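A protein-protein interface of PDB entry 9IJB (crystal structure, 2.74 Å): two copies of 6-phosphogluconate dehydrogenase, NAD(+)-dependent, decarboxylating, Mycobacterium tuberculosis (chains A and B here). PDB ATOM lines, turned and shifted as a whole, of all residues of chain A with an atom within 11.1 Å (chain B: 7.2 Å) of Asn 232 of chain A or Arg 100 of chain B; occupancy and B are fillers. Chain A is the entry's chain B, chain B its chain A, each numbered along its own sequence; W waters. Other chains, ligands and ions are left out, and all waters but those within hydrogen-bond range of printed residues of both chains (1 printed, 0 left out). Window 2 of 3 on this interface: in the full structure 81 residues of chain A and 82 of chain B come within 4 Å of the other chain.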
ATOM      1  N   ASN A 213     -27.012   4.243  16.177  1.00  0.00           N
ATOM      2  CA  ASN A 213     -26.592   2.883  15.935  1.00  0.00           C
ATOM      3  C   ASN A 213     -26.661   1.966  17.117  1.00  0.00           C
ATOM      4  O   ASN A 213     -26.038   0.949  17.131  1.00  0.00           O
ATOM      5  CB  ASN A 213     -25.209   2.844  15.319  1.00  0.00           C
ATOM      6  CG  ASN A 213     -25.178   3.430  13.939  1.00  0.00           C
ATOM      7  OD1 ASN A 213     -24.707   4.515  13.741  1.00  0.00           O
ATOM      8  ND2 ASN A 213     -25.701   2.716  12.988  1.00  0.00           N
ATOM      9  N   ALA A 214     -27.418   2.347  18.117  1.00  0.00           N
ATOM     10  CA  ALA A 214     -27.576   1.568  19.320  1.00  0.00           C
ATOM     11  C   ALA A 214     -28.444   0.360  19.073  1.00  0.00           C
ATOM     12  O   ALA A 214     -28.578  -0.487  19.907  1.00  0.00           O
ATOM     13  CB  ALA A 214     -28.140   2.415  20.423  1.00  0.00           C
ATOM     14  N   ASP A 215     -29.035   0.297  17.900  1.00  0.00           N
ATOM     15  CA  ASP A 215     -29.892  -0.793  17.492  1.00  0.00           C
ATOM     16  C   ASP A 215     -29.092  -1.809  16.729  1.00  0.00           C
ATOM     17  O   ASP A 215     -29.622  -2.522  15.940  1.00  0.00           O
ATOM     18  CB  ASP A 215     -30.988  -0.280  16.587  1.00  0.00           C
ATOM     19  CG  ASP A 215     -30.454   0.425  15.374  1.00  0.00           C
ATOM     20  OD1 ASP A 215     -29.253   0.360  15.132  1.00  0.00           O
ATOM     21  OD2 ASP A 215     -31.235   1.048  14.645  1.00  0.00           O
ATOM     22  N   VAL A 216     -27.795  -1.847  16.945  1.00  0.00           N
ATOM     23  CA  VAL A 216     -26.899  -2.733  16.221  1.00  0.00           C
ATOM     24  C   VAL A 216     -27.198  -4.223  16.376  1.00  0.00           C
ATOM     25  O   VAL A 216     -27.046  -4.976  15.436  1.00  0.00           O
ATOM     26  CB  VAL A 216     -25.424  -2.361  16.511  1.00  0.00           C
ATOM     27  CG1 VAL A 216     -24.887  -2.998  17.774  1.00  0.00           C
ATOM     28  CG2 VAL A 216     -24.541  -2.656  15.325  1.00  0.00           C
ATOM     29  N   GLY A 217     -27.617  -4.636  17.557  1.00  0.00           N
ATOM     30  CA  GLY A 217     -27.916  -6.027  17.835  1.00  0.00           C
ATOM     31  C   GLY A 217     -29.013  -6.567  16.953  1.00  0.00           C
ATOM     32  O   GLY A 217     -28.996  -7.703  16.550  1.00  0.00           O
ATOM     33  N   THR A 218     -29.996  -5.745  16.672  1.00  0.00           N
ATOM     34  CA  THR A 218     -31.096  -6.134  15.786  1.00  0.00           C
ATOM     35  C   THR A 218     -30.621  -6.329  14.342  1.00  0.00           C
ATOM     36  O   THR A 218     -31.109  -7.220  13.638  1.00  0.00           O
ATOM     37  CB  THR A 218     -32.229  -5.095  15.825  1.00  0.00           C
ATOM     38  OG1 THR A 218     -31.909  -3.995  14.958  1.00  0.00           O
ATOM     39  CG2 THR A 218     -32.516  -4.590  17.276  1.00  0.00           C
ATOM     40  N   ARG A 219     -29.686  -5.504  13.869  1.00  0.00           N
ATOM     41  CA  ARG A 219     -29.367  -5.893  12.492  1.00  0.00           C
ATOM     42  C   ARG A 219     -28.146  -6.819  12.479  1.00  0.00           C
ATOM     43  O   ARG A 219     -28.089  -7.790  11.721  1.00  0.00           O
ATOM     44  CB  ARG A 219     -29.130  -4.665  11.582  1.00  0.00           C
ATOM     45  CG  ARG A 219     -30.316  -3.651  11.477  1.00  0.00           C
ATOM     46  CD  ARG A 219     -30.009  -2.409  10.580  1.00  0.00           C
ATOM     47  NE  ARG A 219     -29.097  -1.435  11.205  1.00  0.00           N
ATOM     48  CZ  ARG A 219     -29.449  -0.543  12.142  1.00  0.00           C
ATOM     49  NH1 ARG A 219     -30.701  -0.503  12.610  1.00  0.00           N
ATOM     50  NH2 ARG A 219     -28.537   0.315  12.615  1.00  0.00           N
ATOM     51  N   ALA A 228     -14.860  -8.056  13.648  1.00  0.00           N
ATOM     52  CA  ALA A 228     -15.957  -7.188  14.037  1.00  0.00           C
ATOM     53  C   ALA A 228     -17.238  -7.912  14.515  1.00  0.00           C
ATOM     54  O   ALA A 228     -18.341  -7.425  14.247  1.00  0.00           O
ATOM     55  CB  ALA A 228     -16.301  -6.264  12.859  1.00  0.00           C
ATOM     56  N   PRO A 229     -17.128  -9.040  15.229  1.00  0.00           N
ATOM     57  CA  PRO A 229     -18.343  -9.662  15.763  1.00  0.00           C
ATOM     58  C   PRO A 229     -18.802  -8.941  17.018  1.00  0.00           C
ATOM     59  O   PRO A 229     -18.015  -8.317  17.738  1.00  0.00           O
ATOM     60  CB  PRO A 229     -17.896 -11.091  16.075  1.00  0.00           C
ATOM     61  CG  PRO A 229     -16.503 -10.903  16.544  1.00  0.00           C
ATOM     62  CD  PRO A 229     -15.932  -9.734  15.744  1.00  0.00           C
ATOM     63  N   LEU A 230     -20.097  -9.023  17.254  1.00  0.00           N
ATOM     64  CA  LEU A 230     -20.664  -8.360  18.386  1.00  0.00           C
ATOM     65  C   LEU A 230     -21.107  -9.317  19.447  1.00  0.00           C
ATOM     66  O   LEU A 230     -21.942 -10.186  19.230  1.00  0.00           O
ATOM     67  CB  LEU A 230     -21.859  -7.525  17.942  1.00  0.00           C
ATOM     68  CG  LEU A 230     -22.642  -6.800  19.019  1.00  0.00           C
ATOM     69  CD1 LEU A 230     -21.738  -5.790  19.660  1.00  0.00           C
ATOM     70  CD2 LEU A 230     -23.855  -6.115  18.440  1.00  0.00           C
ATOM     71  N   PRO A 231     -20.486  -9.112  20.659  1.00  0.00           N
ATOM     72  CA  PRO A 231     -20.979  -9.961  21.732  1.00  0.00           C
ATOM     73  C   PRO A 231     -22.066  -9.152  22.421  1.00  0.00           C
ATOM     74  O   PRO A 231     -22.071  -7.930  22.301  1.00  0.00           O
ATOM     75  CB  PRO A 231     -19.781 -10.088  22.638  1.00  0.00           C
ATOM     76  CG  PRO A 231     -19.226  -8.728  22.640  1.00  0.00           C
ATOM     77  CD  PRO A 231     -19.336  -8.274  21.224  1.00  0.00           C
ATOM     78  N   ASN A 232     -22.952  -9.795  23.159  1.00  0.00           N
ATOM     79  CA  ASN A 232     -23.975  -9.045  23.833  1.00  0.00           C
ATOM     80  C   ASN A 232     -24.868  -8.283  22.883  1.00  0.00           C
ATOM     81  O   ASN A 232     -25.119  -7.101  23.055  1.00  0.00           O
ATOM     82  CB  ASN A 232     -23.283  -8.076  24.767  1.00  0.00           C
ATOM     83  CG  ASN A 232     -22.259  -8.756  25.631  1.00  0.00           C
ATOM     84  OD1 ASN A 232     -21.161  -8.245  25.830  1.00  0.00           O
ATOM     85  ND2 ASN A 232     -22.610  -9.918  26.152  1.00  0.00           N
ATOM     86  N   PRO A 233     -25.380  -9.030  21.837  1.00  0.00           N
ATOM     87  CA  PRO A 233     -26.278  -8.287  20.947  1.00  0.00           C
ATOM     88  C   PRO A 233     -27.455  -7.805  21.777  1.00  0.00           C
ATOM     89  O   PRO A 233     -28.110  -6.857  21.416  1.00  0.00           O
ATOM     90  CB  PRO A 233     -26.727  -9.323  19.924  1.00  0.00           C
ATOM     91  CG  PRO A 233     -26.595 -10.605  20.615  1.00  0.00           C
ATOM     92  CD  PRO A 233     -25.297 -10.454  21.299  1.00  0.00           C
ATOM     93  N   GLU A 234     -27.726  -8.479  22.877  1.00  0.00           N
ATOM     94  CA  GLU A 234     -28.809  -8.102  23.787  1.00  0.00           C
ATOM     95  C   GLU A 234     -28.574  -6.764  24.491  1.00  0.00           C
ATOM     96  O   GLU A 234     -29.484  -6.278  25.169  1.00  0.00           O
ATOM     97  CB  GLU A 234     -29.041  -9.186  24.836  1.00  0.00           C
ATOM     98  CG  GLU A 234     -27.916  -9.315  25.835  1.00  0.00           C
ATOM     99  CD  GLU A 234     -26.738 -10.107  25.298  1.00  0.00           C
ATOM    100  OE1 GLU A 234     -25.722 -10.250  26.027  1.00  0.00           O
ATOM    101  OE2 GLU A 234     -26.834 -10.582  24.146  1.00  0.00           O
ATOM    102  N   CYS A 235     -27.385  -6.166  24.353  1.00  0.00           N
ATOM    103  CA  CYS A 235     -27.087  -4.872  24.943  1.00  0.00           C
ATOM    104  C   CYS A 235     -27.262  -3.720  23.960  1.00  0.00           C
ATOM    105  O   CYS A 235     -27.147  -2.560  24.361  1.00  0.00           O
ATOM    106  CB  CYS A 235     -25.655  -4.878  25.507  1.00  0.00           C
ATOM    107  SG  CYS A 235     -25.469  -5.977  26.940  1.00  0.00           S
ATOM    108  N   TYR A 236     -27.568  -4.004  22.693  1.00  0.00           N
ATOM    109  CA  TYR A 236     -27.691  -2.977  21.651  1.00  0.00           C
ATOM    110  C   TYR A 236     -29.018  -3.271  20.948  1.00  0.00           C
ATOM    111  O   TYR A 236     -29.056  -3.814  19.836  1.00  0.00           O
ATOM    112  CB  TYR A 236     -26.448  -2.955  20.756  1.00  0.00           C
ATOM    113  CG  TYR A 236     -25.180  -2.563  21.473  1.00  0.00           C
ATOM    114  CD1 TYR A 236     -24.892  -1.220  21.756  1.00  0.00           C
ATOM    115  CD2 TYR A 236     -24.255  -3.531  21.873  1.00  0.00           C
ATOM    116  CE1 TYR A 236     -23.717  -0.851  22.413  1.00  0.00           C
ATOM    117  CE2 TYR A 236     -23.075  -3.166  22.536  1.00  0.00           C
ATOM    118  CZ  TYR A 236     -22.823  -1.832  22.803  1.00  0.00           C
ATOM    119  OH  TYR A 236     -21.681  -1.483  23.472  1.00  0.00           O
ATOM    120  N   GLN A 237     -30.122  -2.873  21.597  1.00  0.00           N
ATOM    121  CA  GLN A 237     -31.470  -3.143  21.101  1.00  0.00           C
ATOM    122  C   GLN A 237     -32.354  -1.906  21.013  1.00  0.00           C
ATOM    123  O   GLN A 237     -33.585  -2.034  21.035  1.00  0.00           O
ATOM    124  CB  GLN A 237     -32.182  -4.178  21.977  1.00  0.00           C
ATOM    125  CG  GLN A 237     -32.428  -3.677  23.393  1.00  0.00           C
ATOM    126  CD  GLN A 237     -32.959  -4.759  24.289  1.00  0.00           C
ATOM    127  OE1 GLN A 237     -33.033  -5.940  23.916  1.00  0.00           O
ATOM    128  NE2 GLN A 237     -33.258  -4.395  25.512  1.00  0.00           N
ATOM    129  N   TYR A 238     -31.781  -0.718  20.937  1.00  0.00           N
ATOM    130  CA  TYR A 238     -32.570   0.488  21.102  1.00  0.00           C
ATOM    131  C   TYR A 238     -32.712   1.271  19.809  1.00  0.00           C
ATOM    132  O   TYR A 238     -31.716   1.554  19.132  1.00  0.00           O
ATOM    133  CB  TYR A 238     -31.960   1.360  22.191  1.00  0.00           C
ATOM    134  CG  TYR A 238     -31.795   0.690  23.540  1.00  0.00           C
ATOM    135  CD1 TYR A 238     -32.838   0.031  24.165  1.00  0.00           C
ATOM    136  CD2 TYR A 238     -30.589   0.762  24.201  1.00  0.00           C
ATOM    137  CE1 TYR A 238     -32.662  -0.554  25.403  1.00  0.00           C
ATOM    138  CE2 TYR A 238     -30.413   0.186  25.431  1.00  0.00           C
ATOM    139  CZ  TYR A 238     -31.438  -0.463  26.025  1.00  0.00           C
ATOM    140  OH  TYR A 238     -31.195  -1.014  27.254  1.00  0.00           O
ATOM    141  N   PHE A 240     -33.632   4.723  19.062  1.00  0.00           N
ATOM    142  CA  PHE A 240     -33.848   6.030  19.642  1.00  0.00           C
ATOM    143  C   PHE A 240     -34.441   7.004  18.638  1.00  0.00           C
ATOM    144  O   PHE A 240     -34.091   6.987  17.450  1.00  0.00           O
ATOM    145  CB  PHE A 240     -32.535   6.569  20.195  1.00  0.00           C
ATOM    146  CG  PHE A 240     -32.030   5.804  21.364  1.00  0.00           C
ATOM    147  CD1 PHE A 240     -32.768   5.741  22.539  1.00  0.00           C
ATOM    148  CD2 PHE A 240     -30.826   5.129  21.291  1.00  0.00           C
ATOM    149  CE1 PHE A 240     -32.303   5.018  23.623  1.00  0.00           C
ATOM    150  CE2 PHE A 240     -30.355   4.395  22.379  1.00  0.00           C
ATOM    151  CZ  PHE A 240     -31.096   4.342  23.548  1.00  0.00           C
ATOM    152  N   THR B  97     -26.724   4.675  37.191  1.00  0.00           N
ATOM    153  CA  THR B  97     -26.618   3.239  36.979  1.00  0.00           C
ATOM    154  C   THR B  97     -26.217   2.929  35.535  1.00  0.00           C
ATOM    155  O   THR B  97     -26.616   3.629  34.597  1.00  0.00           O
ATOM    156  CB  THR B  97     -27.946   2.549  37.326  1.00  0.00           C
ATOM    157  OG1 THR B  97     -28.230   2.705  38.729  1.00  0.00           O
ATOM    158  CG2 THR B  97     -27.893   1.048  36.978  1.00  0.00           C
ATOM    159  N   TYR B  98     -25.408   1.882  35.363  1.00  0.00           N
ATOM    160  CA  TYR B  98     -25.052   1.402  34.032  1.00  0.00           C
ATOM    161  C   TYR B  98     -26.242   0.699  33.394  1.00  0.00           C
ATOM    162  O   TYR B  98     -26.889  -0.138  34.028  1.00  0.00           O
ATOM    163  CB  TYR B  98     -23.870   0.445  34.125  1.00  0.00           C
ATOM    164  CG  TYR B  98     -23.194   0.102  32.815  1.00  0.00           C
ATOM    165  CD1 TYR B  98     -23.163   1.002  31.749  1.00  0.00           C
ATOM    166  CD2 TYR B  98     -22.572  -1.137  32.652  1.00  0.00           C
ATOM    167  CE1 TYR B  98     -22.523   0.662  30.542  1.00  0.00           C
ATOM    168  CE2 TYR B  98     -21.938  -1.483  31.469  1.00  0.00           C
ATOM    169  CZ  TYR B  98     -21.912  -0.584  30.420  1.00  0.00           C
ATOM    170  OH  TYR B  98     -21.268  -0.945  29.265  1.00  0.00           O
ATOM    171  N   TYR B  99     -26.521   1.025  32.129  1.00  0.00           N
ATOM    172  CA  TYR B  99     -27.752   0.540  31.515  1.00  0.00           C
ATOM    173  C   TYR B  99     -27.790  -0.981  31.470  1.00  0.00           C
ATOM    174  O   TYR B  99     -28.874  -1.579  31.553  1.00  0.00           O
ATOM    175  CB  TYR B  99     -27.929   1.151  30.126  1.00  0.00           C
ATOM    176  CG  TYR B  99     -27.199   0.483  28.994  1.00  0.00           C
ATOM    177  CD1 TYR B  99     -25.882   0.808  28.709  1.00  0.00           C
ATOM    178  CD2 TYR B  99     -27.842  -0.440  28.165  1.00  0.00           C
ATOM    179  CE1 TYR B  99     -25.221   0.234  27.660  1.00  0.00           C
ATOM    180  CE2 TYR B  99     -27.187  -1.016  27.109  1.00  0.00           C
ATOM    181  CZ  TYR B  99     -25.872  -0.678  26.855  1.00  0.00           C
ATOM    182  OH  TYR B  99     -25.193  -1.252  25.797  1.00  0.00           O
ATOM    183  N   ARG B 100     -26.622  -1.620  31.379  1.00  0.00           N
ATOM    184  CA  ARG B 100     -26.644  -3.074  31.383  1.00  0.00           C
ATOM    185  C   ARG B 100     -27.096  -3.609  32.739  1.00  0.00           C
ATOM    186  O   ARG B 100     -27.687  -4.687  32.806  1.00  0.00           O
ATOM    187  CB  ARG B 100     -25.269  -3.618  30.988  1.00  0.00           C
ATOM    188  CG  ARG B 100     -24.761  -3.096  29.621  1.00  0.00           C
ATOM    189  CD  ARG B 100     -23.889  -4.142  28.953  1.00  0.00           C
ATOM    190  NE  ARG B 100     -22.838  -3.590  28.099  1.00  0.00           N
ATOM    191  CZ  ARG B 100     -21.967  -4.329  27.408  1.00  0.00           C
ATOM    192  NH1 ARG B 100     -22.016  -5.658  27.468  1.00  0.00           N
ATOM    193  NH2 ARG B 100     -21.039  -3.747  26.658  1.00  0.00           N
ATOM    194  N   ASP B 101     -26.935  -2.835  33.818  1.00  0.00           N
ATOM    195  CA  ASP B 101     -27.426  -3.274  35.123  1.00  0.00           C
ATOM    196  C   ASP B 101     -28.945  -3.160  35.195  1.00  0.00           C
ATOM    197  O   ASP B 101     -29.607  -3.993  35.828  1.00  0.00           O
ATOM    198  CB  ASP B 101     -26.773  -2.463  36.246  1.00  0.00           C
ATOM    199  CG  ASP B 101     -25.256  -2.649  36.321  1.00  0.00           C
ATOM    200  OD1 ASP B 101     -24.745  -3.661  35.813  1.00  0.00           O
ATOM    201  OD2 ASP B 101     -24.569  -1.773  36.886  1.00  0.00           O
ATOM    202  N   ASP B 102     -29.513  -2.139  34.548  1.00  0.00           N
ATOM    203  CA  ASP B 102     -30.963  -1.972  34.543  1.00  0.00           C
ATOM    204  C   ASP B 102     -31.678  -3.178  33.960  1.00  0.00           C
ATOM    205  O   ASP B 102     -32.864  -3.379  34.246  1.00  0.00           O
ATOM    206  CB  ASP B 102     -31.353  -0.724  33.756  1.00  0.00           C
ATOM    207  CG  ASP B 102     -31.195   0.543  34.553  1.00  0.00           C
ATOM    208  OD1 ASP B 102     -31.016   0.488  35.794  1.00  0.00           O
ATOM    209  OD2 ASP B 102     -31.262   1.608  33.922  1.00  0.00           O
ATOM    210  N   LEU B 103     -30.989  -3.975  33.144  1.00  0.00           N
ATOM    211  CA  LEU B 103     -31.627  -5.134  32.550  1.00  0.00           C
ATOM    212  C   LEU B 103     -31.716  -6.280  33.548  1.00  0.00           C
ATOM    213  O   LEU B 103     -32.708  -7.018  33.543  1.00  0.00           O
ATOM    214  CB  LEU B 103     -30.880  -5.528  31.280  1.00  0.00           C
ATOM    215  CG  LEU B 103     -31.097  -4.513  30.143  1.00  0.00           C
ATOM    216  CD1 LEU B 103     -30.224  -4.789  28.935  1.00  0.00           C
ATOM    217  CD2 LEU B 103     -32.560  -4.526  29.745  1.00  0.00           C
ATOM    218  N   ARG B 104     -30.737  -6.416  34.448  1.00  0.00           N
ATOM    219  CA  ARG B 104     -30.877  -7.402  35.516  1.00  0.00           C
ATOM    220  C   ARG B 104     -31.959  -6.990  36.504  1.00  0.00           C
ATOM    221  O   ARG B 104     -32.744  -7.831  36.956  1.00  0.00           O
ATOM    222  CB  ARG B 104     -29.545  -7.611  36.232  1.00  0.00           C
ATOM    223  CG  ARG B 104     -28.369  -7.704  35.281  1.00  0.00           C
ATOM    224  CD  ARG B 104     -27.023  -7.771  36.003  1.00  0.00           C
ATOM    225  NE  ARG B 104     -26.073  -6.795  35.460  1.00  0.00           N
ATOM    226  CZ  ARG B 104     -25.504  -6.882  34.257  1.00  0.00           C
ATOM    227  NH1 ARG B 104     -25.771  -7.917  33.463  1.00  0.00           N
ATOM    228  NH2 ARG B 104     -24.662  -5.935  33.845  1.00  0.00           N
ATOM    229  N   HIS B 105     -32.020  -5.699  36.849  1.00  0.00           N
ATOM    230  CA  HIS B 105     -32.999  -5.227  37.826  1.00  0.00           C
ATOM    231  C   HIS B 105     -34.418  -5.360  37.294  1.00  0.00           C
ATOM    232  O   HIS B 105     -35.334  -5.739  38.037  1.00  0.00           O
ATOM    233  CB  HIS B 105     -32.699  -3.772  38.208  1.00  0.00           C
ATOM    234  CG  HIS B 105     -31.380  -3.588  38.899  1.00  0.00           C
ATOM    235  ND1 HIS B 105     -30.721  -2.374  38.956  1.00  0.00           N
ATOM    236  CD2 HIS B 105     -30.591  -4.472  39.560  1.00  0.00           C
ATOM    237  CE1 HIS B 105     -29.593  -2.519  39.629  1.00  0.00           C
ATOM    238  NE2 HIS B 105     -29.491  -3.782  40.007  1.00  0.00           N
ATOM    239  N   GLY B 184     -33.549   0.444  30.160  1.00  0.00           N
ATOM    240  CA  GLY B 184     -32.169   0.838  29.988  1.00  0.00           C
ATOM    241  C   GLY B 184     -31.950   1.998  29.040  1.00  0.00           C
ATOM    242  O   GLY B 184     -30.923   2.671  29.135  1.00  0.00           O
ATOM    243  N   HIS B 187     -30.989   5.478  30.800  1.00  0.00           N
ATOM    244  CA  HIS B 187     -29.609   5.621  31.245  1.00  0.00           C
ATOM    245  C   HIS B 187     -28.654   5.634  30.069  1.00  0.00           C
ATOM    246  O   HIS B 187     -27.657   6.368  30.088  1.00  0.00           O
ATOM    247  CB  HIS B 187     -29.271   4.508  32.225  1.00  0.00           C
ATOM    248  CG  HIS B 187     -29.916   4.689  33.561  1.00  0.00           C
ATOM    249  ND1 HIS B 187     -30.294   3.635  34.359  1.00  0.00           N
ATOM    250  CD2 HIS B 187     -30.258   5.812  34.236  1.00  0.00           C
ATOM    251  CE1 HIS B 187     -30.838   4.098  35.470  1.00  0.00           C
ATOM    252  NE2 HIS B 187     -30.831   5.416  35.419  1.00  0.00           N
ATOM    253  N   PHE B 188     -28.968   4.862  29.028  1.00  0.00           N
ATOM    254  CA  PHE B 188     -28.131   4.839  27.846  1.00  0.00           C
ATOM    255  C   PHE B 188     -28.015   6.233  27.251  1.00  0.00           C
ATOM    256  O   PHE B 188     -26.914   6.686  26.927  1.00  0.00           O
ATOM    257  CB  PHE B 188     -28.691   3.845  26.820  1.00  0.00           C
ATOM    258  CG  PHE B 188     -27.743   3.553  25.678  1.00  0.00           C
ATOM    259  CD1 PHE B 188     -27.541   4.493  24.667  1.00  0.00           C
ATOM    260  CD2 PHE B 188     -27.005   2.377  25.648  1.00  0.00           C
ATOM    261  CE1 PHE B 188     -26.649   4.253  23.617  1.00  0.00           C
ATOM    262  CE2 PHE B 188     -26.107   2.125  24.608  1.00  0.00           C
ATOM    263  CZ  PHE B 188     -25.936   3.063  23.584  1.00  0.00           C
ATOM    264  N   TRP B 288     -18.182   4.371  29.279  1.00  0.00           N
ATOM    265  CA  TRP B 288     -19.186   3.536  28.634  1.00  0.00           C
ATOM    266  C   TRP B 288     -19.574   4.090  27.291  1.00  0.00           C
ATOM    267  O   TRP B 288     -19.817   3.319  26.347  1.00  0.00           O
ATOM    268  CB  TRP B 288     -20.433   3.427  29.486  1.00  0.00           C
ATOM    269  CG  TRP B 288     -20.154   3.041  30.853  1.00  0.00           C
ATOM    270  CD1 TRP B 288     -19.137   2.255  31.294  1.00  0.00           C
ATOM    271  CD2 TRP B 288     -20.910   3.410  32.000  1.00  0.00           C
ATOM    272  NE1 TRP B 288     -19.205   2.122  32.653  1.00  0.00           N
ATOM    273  CE2 TRP B 288     -20.293   2.823  33.110  1.00  0.00           C
ATOM    274  CE3 TRP B 288     -22.060   4.184  32.195  1.00  0.00           C
ATOM    275  CZ2 TRP B 288     -20.777   2.987  34.388  1.00  0.00           C
ATOM    276  CZ3 TRP B 288     -22.532   4.344  33.449  1.00  0.00           C
ATOM    277  CH2 TRP B 288     -21.899   3.749  34.537  1.00  0.00           C
ATOM    278  N   ILE B 291     -17.086   3.012  24.926  1.00  0.00           N
ATOM    279  CA  ILE B 291     -17.096   1.578  24.638  1.00  0.00           C
ATOM    280  C   ILE B 291     -18.286   1.229  23.749  1.00  0.00           C
ATOM    281  O   ILE B 291     -18.160   0.438  22.805  1.00  0.00           O
ATOM    282  CB  ILE B 291     -17.069   0.747  25.936  1.00  0.00           C
ATOM    283  CG1 ILE B 291     -15.803   1.051  26.751  1.00  0.00           C
ATOM    284  CG2 ILE B 291     -17.145  -0.756  25.629  1.00  0.00           C
ATOM    285  CD1 ILE B 291     -15.625   0.148  27.989  1.00  0.00           C
ATOM    286  N   ALA B 292     -19.448   1.847  23.991  1.00  0.00           N
ATOM    287  CA  ALA B 292     -20.563   1.647  23.070  1.00  0.00           C
ATOM    288  C   ALA B 292     -20.151   1.993  21.640  1.00  0.00           C
ATOM    289  O   ALA B 292     -20.412   1.233  20.698  1.00  0.00           O
ATOM    290  CB  ALA B 292     -21.771   2.481  23.495  1.00  0.00           C
ATOM    291  N   ASP B 295     -18.148  -0.659  20.129  1.00  0.00           N
ATOM    292  CA  ASP B 295     -18.987  -1.826  19.865  1.00  0.00           C
ATOM    293  C   ASP B 295     -19.825  -1.635  18.611  1.00  0.00           C
ATOM    294  O   ASP B 295     -20.063  -2.597  17.878  1.00  0.00           O
ATOM    295  CB  ASP B 295     -19.911  -2.110  21.056  1.00  0.00           C
ATOM    296  CG  ASP B 295     -19.297  -3.055  22.081  1.00  0.00           C
ATOM    297  OD1 ASP B 295     -18.304  -3.738  21.756  1.00  0.00           O
ATOM    298  OD2 ASP B 295     -19.809  -3.108  23.231  1.00  0.00           O
HETATM  299  O   HOH W   1     -22.658  -0.440  25.557  1.00  0.00           O
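The side-chain hydroxyl (OH) of Tyr 99 of chain B sits at hydrogen-bond distance from the backbone carbonyl oxygen (O) of Cys 235 of chain A. OD1 of Asn 232 of chain A is in hydrogen-bond range of NH1 of Arg 100 of chain B. The guanidinium group of Arg 100 of chain B lies close to the side-chain sulfur of Cys 235 of chain A, 3.5 Å away. OH of Tyr 236 of chain A lies within hydrogen-bond range of OD2 of Asp 295 of chain B (2.5 Å).
No position is printed for both chains.
Among the printed residues, merely in contact across the chains: Ala 214 of chain A with Phe 188 of chain B, Tyr 236 of chain A with Tyr 99 of chain B, Tyr 236 of chain A with Arg 100 of chain B, Tyr 236 of chain A with Ala 292 of chain B, Tyr 238 of chain A with Tyr 99 of chain B, Tyr 238 of chain A with Gly 184 of chain B and Phe 240 of chain A with Phe 188 of chain B.
OH of Tyr 98 of chain B lies within hydrogen-bond range of NE of Arg 100 of chain B (3.3 Å). O of Arg 100 of chain B sits close to NH2 of Arg 104 of chain B (3.4 Å). The side-chain carboxylate (OD2) of Asp 295 of chain B is in salt-bridge range of the guanidinium group (NH2) of Arg 100 of chain B (3.7 Å). The backbone NH (N) of Tyr 238 of chain A lies within hydrogen-bond range of the backbone carbonyl oxygen (O) of Ala 214 of chain A, 3.4 Å away. The backbone NH of Asp 215 of chain A is in hydrogen-bond range of the backbone carbonyl oxygen of Tyr 238 of chain A, at 3.2 Å. O of Tyr 236 of chain A lies within hydrogen-bond range of N of Gly 217 of chain A, at 2.8 Å.
Of the 16 printed residues of chain B, 6 touch a printed residue of chain A. Hydrophobic or aromatic side chains of chain A that line the printed part of chain B: Ala 214, Tyr 236, Tyr 238 and Phe 240.
Printed residues of chain B within 4 Å of Cys 235 of chain A: Tyr 99 (2.8 Å) and Arg 100 (3.1 Å). Of the printed residues of chain B, Tyr 236 of chain A touches Tyr 99 (3.7 Å), Arg 100 (3.96 Å), Ala 292 (3.3 Å) and Asp 295 (2.5 Å). Of the printed residues of chain B, Tyr 238 of chain A touches Tyr 99 (3.5 Å) and Gly 184 (3.4 Å). No residue of chain A comes within 4 Å of Tyr 98 of chain B. Tyr 99 of chain B touches just these residues of chain A: Cys 235 (2.8 Å), Tyr 236 (3.7 Å) and Tyr 238 (3.5 Å). Of the printed residues of chain A, Arg 100 of chain B touches Asn 232 (3.2 Å), Cys 235 (3.1 Å) and Tyr 236 (3.96 Å). Asp 101 of chain B touches none of the printed residues of chain A. Of the printed residues of chain A, Ala 292 of chain B touches Tyr 236. Of the printed residues of chain A, Asp 295 of chain B touches Tyr 236. The nearest printed residue of chain B that does not touch Tyr 236 of chain A is Ile 291 of chain B (4.1 Å).
Water W1 bridges the side-chain hydroxyl of Tyr 236 of chain A (2.5 Å) and the side-chain hydroxyl of Tyr 99 of chain B (2.7 Å).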
